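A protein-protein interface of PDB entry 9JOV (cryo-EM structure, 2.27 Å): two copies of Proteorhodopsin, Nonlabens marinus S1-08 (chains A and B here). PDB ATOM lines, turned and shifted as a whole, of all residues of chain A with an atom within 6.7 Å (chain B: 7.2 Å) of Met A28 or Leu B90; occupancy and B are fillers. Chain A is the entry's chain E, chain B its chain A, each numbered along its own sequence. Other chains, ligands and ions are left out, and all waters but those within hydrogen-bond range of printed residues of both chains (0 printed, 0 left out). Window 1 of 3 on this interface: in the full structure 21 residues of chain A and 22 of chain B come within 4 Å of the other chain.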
ATOM      1  N   PHE A  23     -32.479 -13.853 -26.959  1.00  0.00           N
ATOM      2  CA  PHE A  23     -33.282 -12.757 -27.488  1.00  0.00           C
ATOM      3  C   PHE A  23     -33.374 -11.617 -26.476  1.00  0.00           C
ATOM      4  O   PHE A  23     -33.231 -10.467 -26.870  1.00  0.00           O
ATOM      5  CB  PHE A  23     -34.695 -13.136 -27.861  1.00  0.00           C
ATOM      6  CG  PHE A  23     -34.839 -13.684 -29.263  1.00  0.00           C
ATOM      7  CD1 PHE A  23     -34.426 -12.925 -30.351  1.00  0.00           C
ATOM      8  CD2 PHE A  23     -35.381 -14.961 -29.479  1.00  0.00           C
ATOM      9  CE1 PHE A  23     -34.548 -13.444 -31.647  1.00  0.00           C
ATOM     10  CE2 PHE A  23     -35.513 -15.475 -30.762  1.00  0.00           C
ATOM     11  CZ  PHE A  23     -35.096 -14.729 -31.845  1.00  0.00           C
ATOM     12  N   PHE A  24     -33.552 -11.928 -25.177  1.00  0.00           N
ATOM     13  CA  PHE A  24     -33.647 -10.890 -24.151  1.00  0.00           C
ATOM     14  C   PHE A  24     -32.332 -10.137 -23.986  1.00  0.00           C
ATOM     15  O   PHE A  24     -32.312  -8.915 -23.897  1.00  0.00           O
ATOM     16  CB  PHE A  24     -34.048 -11.426 -22.794  1.00  0.00           C
ATOM     17  CG  PHE A  24     -35.553 -11.571 -22.601  1.00  0.00           C
ATOM     18  CD1 PHE A  24     -36.215 -12.717 -23.023  1.00  0.00           C
ATOM     19  CD2 PHE A  24     -36.311 -10.526 -22.061  1.00  0.00           C
ATOM     20  CE1 PHE A  24     -37.594 -12.846 -22.889  1.00  0.00           C
ATOM     21  CE2 PHE A  24     -37.683 -10.682 -21.867  1.00  0.00           C
ATOM     22  CZ  PHE A  24     -38.318 -11.853 -22.271  1.00  0.00           C
ATOM     23  N   VAL A  25     -31.211 -10.851 -24.034  1.00  0.00           N
ATOM     24  CA  VAL A  25     -29.930 -10.209 -23.841  1.00  0.00           C
ATOM     25  C   VAL A  25     -29.616  -9.323 -25.030  1.00  0.00           C
ATOM     26  O   VAL A  25     -29.169  -8.196 -24.847  1.00  0.00           O
ATOM     27  CB  VAL A  25     -28.798 -11.209 -23.573  1.00  0.00           C
ATOM     28  CG1 VAL A  25     -27.489 -10.460 -23.378  1.00  0.00           C
ATOM     29  CG2 VAL A  25     -29.054 -11.982 -22.310  1.00  0.00           C
ATOM     30  N   GLY A  26     -29.821  -9.859 -26.239  1.00  0.00           N
ATOM     31  CA  GLY A  26     -29.541  -9.132 -27.457  1.00  0.00           C
ATOM     32  C   GLY A  26     -30.369  -7.848 -27.563  1.00  0.00           C
ATOM     33  O   GLY A  26     -29.849  -6.744 -27.760  1.00  0.00           O
ATOM     34  N   CYS A  27     -31.632  -7.946 -27.272  1.00  0.00           N
ATOM     35  CA  CYS A  27     -32.439  -6.736 -27.232  1.00  0.00           C
ATOM     36  C   CYS A  27     -31.851  -5.695 -26.280  1.00  0.00           C
ATOM     37  O   CYS A  27     -31.731  -4.545 -26.683  1.00  0.00           O
ATOM     38  CB  CYS A  27     -33.885  -7.061 -26.874  1.00  0.00           C
ATOM     39  SG  CYS A  27     -34.894  -5.574 -26.982  1.00  0.00           S
ATOM     40  N   MET A  28     -31.480  -6.086 -25.030  1.00  0.00           N
ATOM     41  CA  MET A  28     -30.993  -5.130 -24.045  1.00  0.00           C
ATOM     42  C   MET A  28     -29.625  -4.555 -24.434  1.00  0.00           C
ATOM     43  O   MET A  28     -29.369  -3.364 -24.276  1.00  0.00           O
ATOM     44  CB  MET A  28     -30.835  -5.738 -22.649  1.00  0.00           C
ATOM     45  CG  MET A  28     -32.106  -6.068 -21.920  1.00  0.00           C
ATOM     46  SD  MET A  28     -33.109  -4.650 -21.444  1.00  0.00           S
ATOM     47  CE  MET A  28     -34.077  -4.473 -22.967  1.00  0.00           C
ATOM     48  N   ALA A  29     -28.728  -5.399 -24.949  1.00  0.00           N
ATOM     49  CA  ALA A  29     -27.423  -4.911 -25.348  1.00  0.00           C
ATOM     50  C   ALA A  29     -27.535  -3.915 -26.524  1.00  0.00           C
ATOM     51  O   ALA A  29     -26.811  -2.925 -26.567  1.00  0.00           O
ATOM     52  CB  ALA A  29     -26.542  -6.101 -25.677  1.00  0.00           C
ATOM     53  N   MET A  30     -28.396  -4.182 -27.506  1.00  0.00           N
ATOM     54  CA  MET A  30     -28.519  -3.237 -28.613  1.00  0.00           C
ATOM     55  C   MET A  30     -29.131  -1.926 -28.122  1.00  0.00           C
ATOM     56  O   MET A  30     -28.704  -0.829 -28.495  1.00  0.00           O
ATOM     57  CB  MET A  30     -29.475  -3.721 -29.698  1.00  0.00           C
ATOM     58  CG  MET A  30     -29.115  -4.993 -30.409  1.00  0.00           C
ATOM     59  SD  MET A  30     -27.594  -4.854 -31.325  1.00  0.00           S
ATOM     60  CE  MET A  30     -27.866  -6.410 -32.171  1.00  0.00           C
ATOM     61  N   MET A  31     -30.143  -2.014 -27.268  1.00  0.00           N
ATOM     62  CA  MET A  31     -30.735  -0.812 -26.701  1.00  0.00           C
ATOM     63  C   MET A  31     -29.689   0.052 -25.996  1.00  0.00           C
ATOM     64  O   MET A  31     -29.640   1.265 -26.205  1.00  0.00           O
ATOM     65  CB  MET A  31     -31.838  -1.158 -25.722  1.00  0.00           C
ATOM     66  CG  MET A  31     -32.490   0.094 -25.129  1.00  0.00           C
ATOM     67  SD  MET A  31     -33.504  -0.481 -23.742  1.00  0.00           S
ATOM     68  CE  MET A  31     -32.337  -0.905 -22.417  1.00  0.00           C
ATOM     69  N   ALA A  32     -28.818  -0.581 -25.205  1.00  0.00           N
ATOM     70  CA  ALA A  32     -27.832   0.149 -24.459  1.00  0.00           C
ATOM     71  C   ALA A  32     -26.758   0.742 -25.368  1.00  0.00           C
ATOM     72  O   ALA A  32     -26.330   1.884 -25.204  1.00  0.00           O
ATOM     73  CB  ALA A  32     -27.236  -0.772 -23.402  1.00  0.00           C
ATOM     74  N   ALA A  33     -26.287  -0.050 -26.333  1.00  0.00           N
ATOM     75  CA  ALA A  33     -25.356   0.441 -27.344  1.00  0.00           C
ATOM     76  C   ALA A  33     -25.947   1.640 -28.103  1.00  0.00           C
ATOM     77  O   ALA A  33     -25.315   2.691 -28.255  1.00  0.00           O
ATOM     78  CB  ALA A  33     -25.037  -0.681 -28.273  1.00  0.00           C
ATOM     79  N   ALA A  63     -32.099  -2.974 -32.102  1.00  0.00           N
ATOM     80  CA  ALA A  63     -32.842  -3.027 -30.827  1.00  0.00           C
ATOM     81  C   ALA A  63     -34.343  -3.133 -31.053  1.00  0.00           C
ATOM     82  O   ALA A  63     -35.008  -3.986 -30.429  1.00  0.00           O
ATOM     83  CB  ALA A  63     -32.581  -1.791 -29.976  1.00  0.00           C
ATOM     84  N   TYR A  66     -35.199  -6.532 -32.582  1.00  0.00           N
ATOM     85  CA  TYR A  66     -35.038  -7.593 -31.570  1.00  0.00           C
ATOM     86  C   TYR A  66     -36.169  -7.581 -30.557  1.00  0.00           C
ATOM     87  O   TYR A  66     -36.584  -8.652 -30.123  1.00  0.00           O
ATOM     88  CB  TYR A  66     -33.754  -7.572 -30.738  1.00  0.00           C
ATOM     89  CG  TYR A  66     -32.765  -8.492 -31.437  1.00  0.00           C
ATOM     90  CD1 TYR A  66     -32.293  -8.199 -32.713  1.00  0.00           C
ATOM     91  CD2 TYR A  66     -32.406  -9.713 -30.871  1.00  0.00           C
ATOM     92  CE1 TYR A  66     -31.434  -9.058 -33.379  1.00  0.00           C
ATOM     93  CE2 TYR A  66     -31.573 -10.600 -31.537  1.00  0.00           C
ATOM     94  CZ  TYR A  66     -31.101 -10.275 -32.802  1.00  0.00           C
ATOM     95  OH  TYR A  66     -30.264 -11.105 -33.490  1.00  0.00           O
ATOM     96  N   ARG A  70     -38.169 -11.018 -30.035  1.00  0.00           N
ATOM     97  CA  ARG A  70     -38.224 -11.574 -28.681  1.00  0.00           C
ATOM     98  C   ARG A  70     -39.651 -11.894 -28.271  1.00  0.00           C
ATOM     99  O   ARG A  70     -39.905 -12.964 -27.724  1.00  0.00           O
ATOM    100  CB  ARG A  70     -37.765 -10.541 -27.651  1.00  0.00           C
ATOM    101  CG  ARG A  70     -37.803 -11.041 -26.218  1.00  0.00           C
ATOM    102  CD  ARG A  70     -37.528  -9.862 -25.320  1.00  0.00           C
ATOM    103  NE  ARG A  70     -38.695  -9.014 -25.172  1.00  0.00           N
ATOM    104  CZ  ARG A  70     -38.741  -7.853 -24.534  1.00  0.00           C
ATOM    105  NH1 ARG A  70     -37.663  -7.213 -24.123  1.00  0.00           N
ATOM    106  NH2 ARG A  70     -39.924  -7.304 -24.338  1.00  0.00           N
ATOM    107  N   ILE B  58     -25.886   1.530 -17.040  1.00  0.00           N
ATOM    108  CA  ILE B  58     -26.145   0.533 -16.023  1.00  0.00           C
ATOM    109  C   ILE B  58     -27.559   0.668 -15.466  1.00  0.00           C
ATOM    110  O   ILE B  58     -28.332  -0.285 -15.514  1.00  0.00           O
ATOM    111  CB  ILE B  58     -25.056   0.542 -14.932  1.00  0.00           C
ATOM    112  CG1 ILE B  58     -23.713   0.050 -15.447  1.00  0.00           C
ATOM    113  CG2 ILE B  58     -25.433  -0.335 -13.757  1.00  0.00           C
ATOM    114  CD1 ILE B  58     -22.510   0.635 -14.737  1.00  0.00           C
ATOM    115  N   PHE B  60     -30.062   2.197 -16.841  1.00  0.00           N
ATOM    116  CA  PHE B  60     -31.046   2.078 -17.924  1.00  0.00           C
ATOM    117  C   PHE B  60     -31.393   0.641 -18.254  1.00  0.00           C
ATOM    118  O   PHE B  60     -32.557   0.266 -18.321  1.00  0.00           O
ATOM    119  CB  PHE B  60     -30.483   2.838 -19.120  1.00  0.00           C
ATOM    120  CG  PHE B  60     -31.310   2.863 -20.382  1.00  0.00           C
ATOM    121  CD1 PHE B  60     -32.680   3.026 -20.331  1.00  0.00           C
ATOM    122  CD2 PHE B  60     -30.711   2.687 -21.632  1.00  0.00           C
ATOM    123  CE1 PHE B  60     -33.433   3.006 -21.501  1.00  0.00           C
ATOM    124  CE2 PHE B  60     -31.463   2.716 -22.805  1.00  0.00           C
ATOM    125  CZ  PHE B  60     -32.826   2.861 -22.733  1.00  0.00           C
ATOM    126  N   ILE B  61     -30.372  -0.216 -18.341  1.00  0.00           N
ATOM    127  CA  ILE B  61     -30.622  -1.625 -18.588  1.00  0.00           C
ATOM    128  C   ILE B  61     -31.467  -2.200 -17.481  1.00  0.00           C
ATOM    129  O   ILE B  61     -32.459  -2.852 -17.762  1.00  0.00           O
ATOM    130  CB  ILE B  61     -29.270  -2.367 -18.778  1.00  0.00           C
ATOM    131  CG1 ILE B  61     -28.618  -1.960 -20.100  1.00  0.00           C
ATOM    132  CG2 ILE B  61     -29.466  -3.858 -18.755  1.00  0.00           C
ATOM    133  CD1 ILE B  61     -27.136  -2.184 -20.107  1.00  0.00           C
ATOM    134  N   ALA B  62     -31.074  -1.965 -16.221  1.00  0.00           N
ATOM    135  CA  ALA B  62     -31.845  -2.410 -15.071  1.00  0.00           C
ATOM    136  C   ALA B  62     -33.270  -1.824 -15.048  1.00  0.00           C
ATOM    137  O   ALA B  62     -34.237  -2.567 -14.878  1.00  0.00           O
ATOM    138  CB  ALA B  62     -31.087  -2.098 -13.821  1.00  0.00           C
ATOM    139  N   ALA B  63     -33.475  -0.553 -15.314  1.00  0.00           N
ATOM    140  CA  ALA B  63     -34.855  -0.044 -15.376  1.00  0.00           C
ATOM    141  C   ALA B  63     -35.698  -0.843 -16.362  1.00  0.00           C
ATOM    142  O   ALA B  63     -36.799  -1.273 -16.018  1.00  0.00           O
ATOM    143  CB  ALA B  63     -34.886   1.415 -15.782  1.00  0.00           C
ATOM    144  N   VAL B  64     -35.171  -1.068 -17.585  1.00  0.00           N
ATOM    145  CA  VAL B  64     -35.969  -1.760 -18.587  1.00  0.00           C
ATOM    146  C   VAL B  64     -36.199  -3.221 -18.184  1.00  0.00           C
ATOM    147  O   VAL B  64     -37.319  -3.734 -18.271  1.00  0.00           O
ATOM    148  CB  VAL B  64     -35.408  -1.602 -20.003  1.00  0.00           C
ATOM    149  CG1 VAL B  64     -36.173  -2.439 -20.989  1.00  0.00           C
ATOM    150  CG2 VAL B  64     -35.428  -0.148 -20.441  1.00  0.00           C
ATOM    151  N   HIS B  65     -35.175  -3.919 -17.679  1.00  0.00           N
ATOM    152  CA  HIS B  65     -35.419  -5.287 -17.246  1.00  0.00           C
ATOM    153  C   HIS B  65     -36.328  -5.340 -16.010  1.00  0.00           C
ATOM    154  O   HIS B  65     -37.177  -6.214 -15.915  1.00  0.00           O
ATOM    155  CB  HIS B  65     -34.117  -6.059 -17.067  1.00  0.00           C
ATOM    156  CG  HIS B  65     -34.334  -7.525 -17.098  1.00  0.00           C
ATOM    157  ND1 HIS B  65     -33.950  -8.326 -16.041  1.00  0.00           N
ATOM    158  CD2 HIS B  65     -34.919  -8.339 -18.030  1.00  0.00           C
ATOM    159  CE1 HIS B  65     -34.309  -9.577 -16.325  1.00  0.00           C
ATOM    160  NE2 HIS B  65     -34.924  -9.606 -17.521  1.00  0.00           N
ATOM    161  N   TYR B  66     -36.198  -4.401 -15.066  1.00  0.00           N
ATOM    162  CA  TYR B  66     -37.114  -4.381 -13.919  1.00  0.00           C
ATOM    163  C   TYR B  66     -38.563  -4.167 -14.351  1.00  0.00           C
ATOM    164  O   TYR B  66     -39.456  -4.761 -13.765  1.00  0.00           O
ATOM    165  CB  TYR B  66     -36.827  -3.346 -12.844  1.00  0.00           C
ATOM    166  CG  TYR B  66     -36.008  -4.032 -11.769  1.00  0.00           C
ATOM    167  CD1 TYR B  66     -34.710  -4.439 -12.044  1.00  0.00           C
ATOM    168  CD2 TYR B  66     -36.548  -4.352 -10.523  1.00  0.00           C
ATOM    169  CE1 TYR B  66     -33.953  -5.123 -11.109  1.00  0.00           C
ATOM    170  CE2 TYR B  66     -35.796  -5.037  -9.580  1.00  0.00           C
ATOM    171  CZ  TYR B  66     -34.496  -5.428  -9.876  1.00  0.00           C
ATOM    172  OH  TYR B  66     -33.704  -6.098  -8.978  1.00  0.00           O
ATOM    173  N   TYR B  85     -30.279 -12.850 -14.738  1.00  0.00           N
ATOM    174  CA  TYR B  85     -28.992 -12.798 -15.409  1.00  0.00           C
ATOM    175  C   TYR B  85     -29.052 -12.039 -16.727  1.00  0.00           C
ATOM    176  O   TYR B  85     -28.021 -11.565 -17.162  1.00  0.00           O
ATOM    177  CB  TYR B  85     -28.460 -14.181 -15.714  1.00  0.00           C
ATOM    178  CG  TYR B  85     -27.859 -14.879 -14.511  1.00  0.00           C
ATOM    179  CD1 TYR B  85     -28.665 -15.373 -13.488  1.00  0.00           C
ATOM    180  CD2 TYR B  85     -26.481 -15.048 -14.395  1.00  0.00           C
ATOM    181  CE1 TYR B  85     -28.126 -16.063 -12.411  1.00  0.00           C
ATOM    182  CE2 TYR B  85     -25.929 -15.731 -13.313  1.00  0.00           C
ATOM    183  CZ  TYR B  85     -26.752 -16.251 -12.337  1.00  0.00           C
ATOM    184  OH  TYR B  85     -26.211 -16.885 -11.274  1.00  0.00           O
ATOM    185  N   VAL B  86     -30.233 -11.834 -17.304  1.00  0.00           N
ATOM    186  CA  VAL B  86     -30.372 -11.035 -18.512  1.00  0.00           C
ATOM    187  C   VAL B  86     -29.737  -9.678 -18.289  1.00  0.00           C
ATOM    188  O   VAL B  86     -29.056  -9.174 -19.162  1.00  0.00           O
ATOM    189  CB  VAL B  86     -31.829 -10.844 -18.948  1.00  0.00           C
ATOM    190  CG1 VAL B  86     -31.945  -9.770 -20.006  1.00  0.00           C
ATOM    191  CG2 VAL B  86     -32.453 -12.166 -19.388  1.00  0.00           C
ATOM    192  N   ASP B  87     -29.984  -9.068 -17.130  1.00  0.00           N
ATOM    193  CA  ASP B  87     -29.377  -7.775 -16.820  1.00  0.00           C
ATOM    194  C   ASP B  87     -27.952  -7.957 -16.284  1.00  0.00           C
ATOM    195  O   ASP B  87     -27.048  -7.282 -16.777  1.00  0.00           O
ATOM    196  CB  ASP B  87     -30.323  -6.962 -15.946  1.00  0.00           C
ATOM    197  CG  ASP B  87     -29.730  -6.211 -14.763  1.00  0.00           C
ATOM    198  OD1 ASP B  87     -28.521  -5.918 -14.804  1.00  0.00           O
ATOM    199  OD2 ASP B  87     -30.481  -5.922 -13.800  1.00  0.00           O
ATOM    200  N   TRP B  88     -27.724  -8.838 -15.293  1.00  0.00           N
ATOM    201  CA  TRP B  88     -26.391  -8.991 -14.709  1.00  0.00           C
ATOM    202  C   TRP B  88     -25.286  -9.244 -15.728  1.00  0.00           C
ATOM    203  O   TRP B  88     -24.235  -8.641 -15.601  1.00  0.00           O
ATOM    204  CB  TRP B  88     -26.306 -10.086 -13.642  1.00  0.00           C
ATOM    205  CG  TRP B  88     -27.262  -9.875 -12.500  1.00  0.00           C
ATOM    206  CD1 TRP B  88     -28.029  -8.774 -12.210  1.00  0.00           C
ATOM    207  CD2 TRP B  88     -27.604 -10.873 -11.533  1.00  0.00           C
ATOM    208  NE1 TRP B  88     -28.810  -9.020 -11.109  1.00  0.00           N
ATOM    209  CE2 TRP B  88     -28.571 -10.290 -10.670  1.00  0.00           C
ATOM    210  CE3 TRP B  88     -27.161 -12.185 -11.297  1.00  0.00           C
ATOM    211  CZ2 TRP B  88     -29.101 -10.987  -9.586  1.00  0.00           C
ATOM    212  CZ3 TRP B  88     -27.686 -12.874 -10.220  1.00  0.00           C
ATOM    213  CH2 TRP B  88     -28.688 -12.299  -9.418  1.00  0.00           C
ATOM    214  N   VAL B  89     -25.512 -10.050 -16.760  1.00  0.00           N
ATOM    215  CA  VAL B  89     -24.458 -10.318 -17.735  1.00  0.00           C
ATOM    216  C   VAL B  89     -24.069  -9.034 -18.469  1.00  0.00           C
ATOM    217  O   VAL B  89     -22.952  -8.975 -18.947  1.00  0.00           O
ATOM    218  CB  VAL B  89     -24.730 -11.422 -18.780  1.00  0.00           C
ATOM    219  CG1 VAL B  89     -24.947 -12.768 -18.131  1.00  0.00           C
ATOM    220  CG2 VAL B  89     -25.900 -11.103 -19.703  1.00  0.00           C
ATOM    221  N   LEU B  90     -24.945  -8.011 -18.550  1.00  0.00           N
ATOM    222  CA  LEU B  90     -24.541  -6.762 -19.182  1.00  0.00           C
ATOM    223  C   LEU B  90     -24.028  -5.754 -18.147  1.00  0.00           C
ATOM    224  O   LEU B  90     -23.022  -5.100 -18.372  1.00  0.00           O
ATOM    225  CB  LEU B  90     -25.658  -6.167 -20.033  1.00  0.00           C
ATOM    226  CG  LEU B  90     -26.204  -7.069 -21.141  1.00  0.00           C
ATOM    227  CD1 LEU B  90     -27.394  -6.426 -21.855  1.00  0.00           C
ATOM    228  CD2 LEU B  90     -25.165  -7.501 -22.143  1.00  0.00           C
ATOM    229  N   THR B  91     -24.721  -5.605 -17.013  1.00  0.00           N
ATOM    230  CA  THR B  91     -24.407  -4.521 -16.096  1.00  0.00           C
ATOM    231  C   THR B  91     -23.140  -4.817 -15.299  1.00  0.00           C
ATOM    232  O   THR B  91     -22.338  -3.893 -15.103  1.00  0.00           O
ATOM    233  CB  THR B  91     -25.597  -4.205 -15.190  1.00  0.00           C
ATOM    234  OG1 THR B  91     -25.972  -5.419 -14.554  1.00  0.00           O
ATOM    235  CG2 THR B  91     -26.772  -3.689 -15.988  1.00  0.00           C
ATOM    236  N   VAL B  92     -22.864  -6.074 -14.918  1.00  0.00           N
ATOM    237  CA  VAL B  92     -21.684  -6.301 -14.084  1.00  0.00           C
ATOM    238  C   VAL B  92     -20.389  -5.970 -14.831  1.00  0.00           C
ATOM    239  O   VAL B  92     -19.502  -5.311 -14.283  1.00  0.00           O
ATOM    240  CB  VAL B  92     -21.654  -7.690 -13.447  1.00  0.00           C
ATOM    241  CG1 VAL B  92     -20.368  -7.932 -12.682  1.00  0.00           C
ATOM    242  CG2 VAL B  92     -22.847  -7.861 -12.535  1.00  0.00           C
ATOM    243  N   PRO B  93     -20.211  -6.352 -16.112  1.00  0.00           N
ATOM    244  CA  PRO B  93     -19.085  -5.858 -16.886  1.00  0.00           C
ATOM    245  C   PRO B  93     -19.010  -4.345 -17.016  1.00  0.00           C
ATOM    246  O   PRO B  93     -17.929  -3.776 -16.814  1.00  0.00           O
ATOM    247  CB  PRO B  93     -19.196  -6.584 -18.225  1.00  0.00           C
ATOM    248  CG  PRO B  93     -20.045  -7.781 -17.909  1.00  0.00           C
ATOM    249  CD  PRO B  93     -20.989  -7.368 -16.820  1.00  0.00           C
ATOM    250  N   LEU B  94     -20.149  -3.669 -17.257  1.00  0.00           N
ATOM    251  CA  LEU B  94     -20.111  -2.205 -17.293  1.00  0.00           C
ATOM    252  C   LEU B  94     -19.638  -1.647 -15.952  1.00  0.00           C
ATOM    253  O   LEU B  94     -18.819  -0.742 -15.924  1.00  0.00           O
ATOM    254  CB  LEU B  94     -21.416  -1.560 -17.726  1.00  0.00           C
ATOM    255  CG  LEU B  94     -21.864  -1.873 -19.161  1.00  0.00           C
ATOM    256  CD1 LEU B  94     -23.281  -1.360 -19.427  1.00  0.00           C
ATOM    257  CD2 LEU B  94     -20.926  -1.249 -20.106  1.00  0.00           C
ATOM    258  N   MET B  95     -20.112  -2.186 -14.834  1.00  0.00           N
ATOM    259  CA  MET B  95     -19.605  -1.732 -13.538  1.00  0.00           C
ATOM    260  C   MET B  95     -18.100  -1.935 -13.421  1.00  0.00           C
ATOM    261  O   MET B  95     -17.407  -0.990 -13.066  1.00  0.00           O
ATOM    262  CB  MET B  95     -20.337  -2.401 -12.375  1.00  0.00           C
ATOM    263  CG  MET B  95     -21.780  -1.898 -12.268  1.00  0.00           C
ATOM    264  SD  MET B  95     -22.833  -2.837 -11.143  1.00  0.00           S
ATOM    265  CE  MET B  95     -22.439  -2.006  -9.610  1.00  0.00           C
ATOM    266  N   LEU B 124     -20.039 -14.063 -14.702  1.00  0.00           N
ATOM    267  CA  LEU B 124     -21.481 -14.118 -14.906  1.00  0.00           C
ATOM    268  C   LEU B 124     -21.908 -15.314 -15.745  1.00  0.00           C
ATOM    269  O   LEU B 124     -22.877 -15.990 -15.391  1.00  0.00           O
ATOM    270  CB  LEU B 124     -22.071 -12.796 -15.401  1.00  0.00           C
ATOM    271  CG  LEU B 124     -22.591 -11.852 -14.300  1.00  0.00           C
ATOM    272  CD1 LEU B 124     -23.589 -12.545 -13.402  1.00  0.00           C
ATOM    273  CD2 LEU B 124     -21.501 -11.366 -13.429  1.00  0.00           C
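Among the printed residues, pairs that only touch across the chains: Ala A29 with Leu B90 (3.5 Å), Met A28 with Val B64 (3.5 Å), Met A31 with Phe B60 (3.6 Å), Ala A32 with Ile B61 (3.6 Å), Met A28 with Leu B90 (3.6 Å), Met A31 with Val B64 (3.7 Å), Phe A24 with Val B86 (3.8 Å) and Val A25 with Leu B90 (3.9 Å).
Printed residues of chain B within 4 Å of Phe A24: Val B86 (3.8 Å).
Met A28 touches just these residues of chain B: Val B64 and Leu B90.
Printed residues of chain B within 4 Å of Met A31: Phe B60 and Val B64.
Printed residues of chain B within 4 Å of Ala A32: Ile B61 (3.6 Å).
Of chain A, only Val A25, Met A28 and Ala A29 come within 4 Å of Leu B90.
The nearest printed residue of chain B that does not touch Met A28 is Ile B61 (4.1 Å).
The nearest printed residue of chain A that does not touch Leu B90 is Ala A32 (5.9 Å).
Of the 14 printed residues of chain A, 6 touch a printed residue of chain B.
Positions printed for both chains: 63 and 66.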
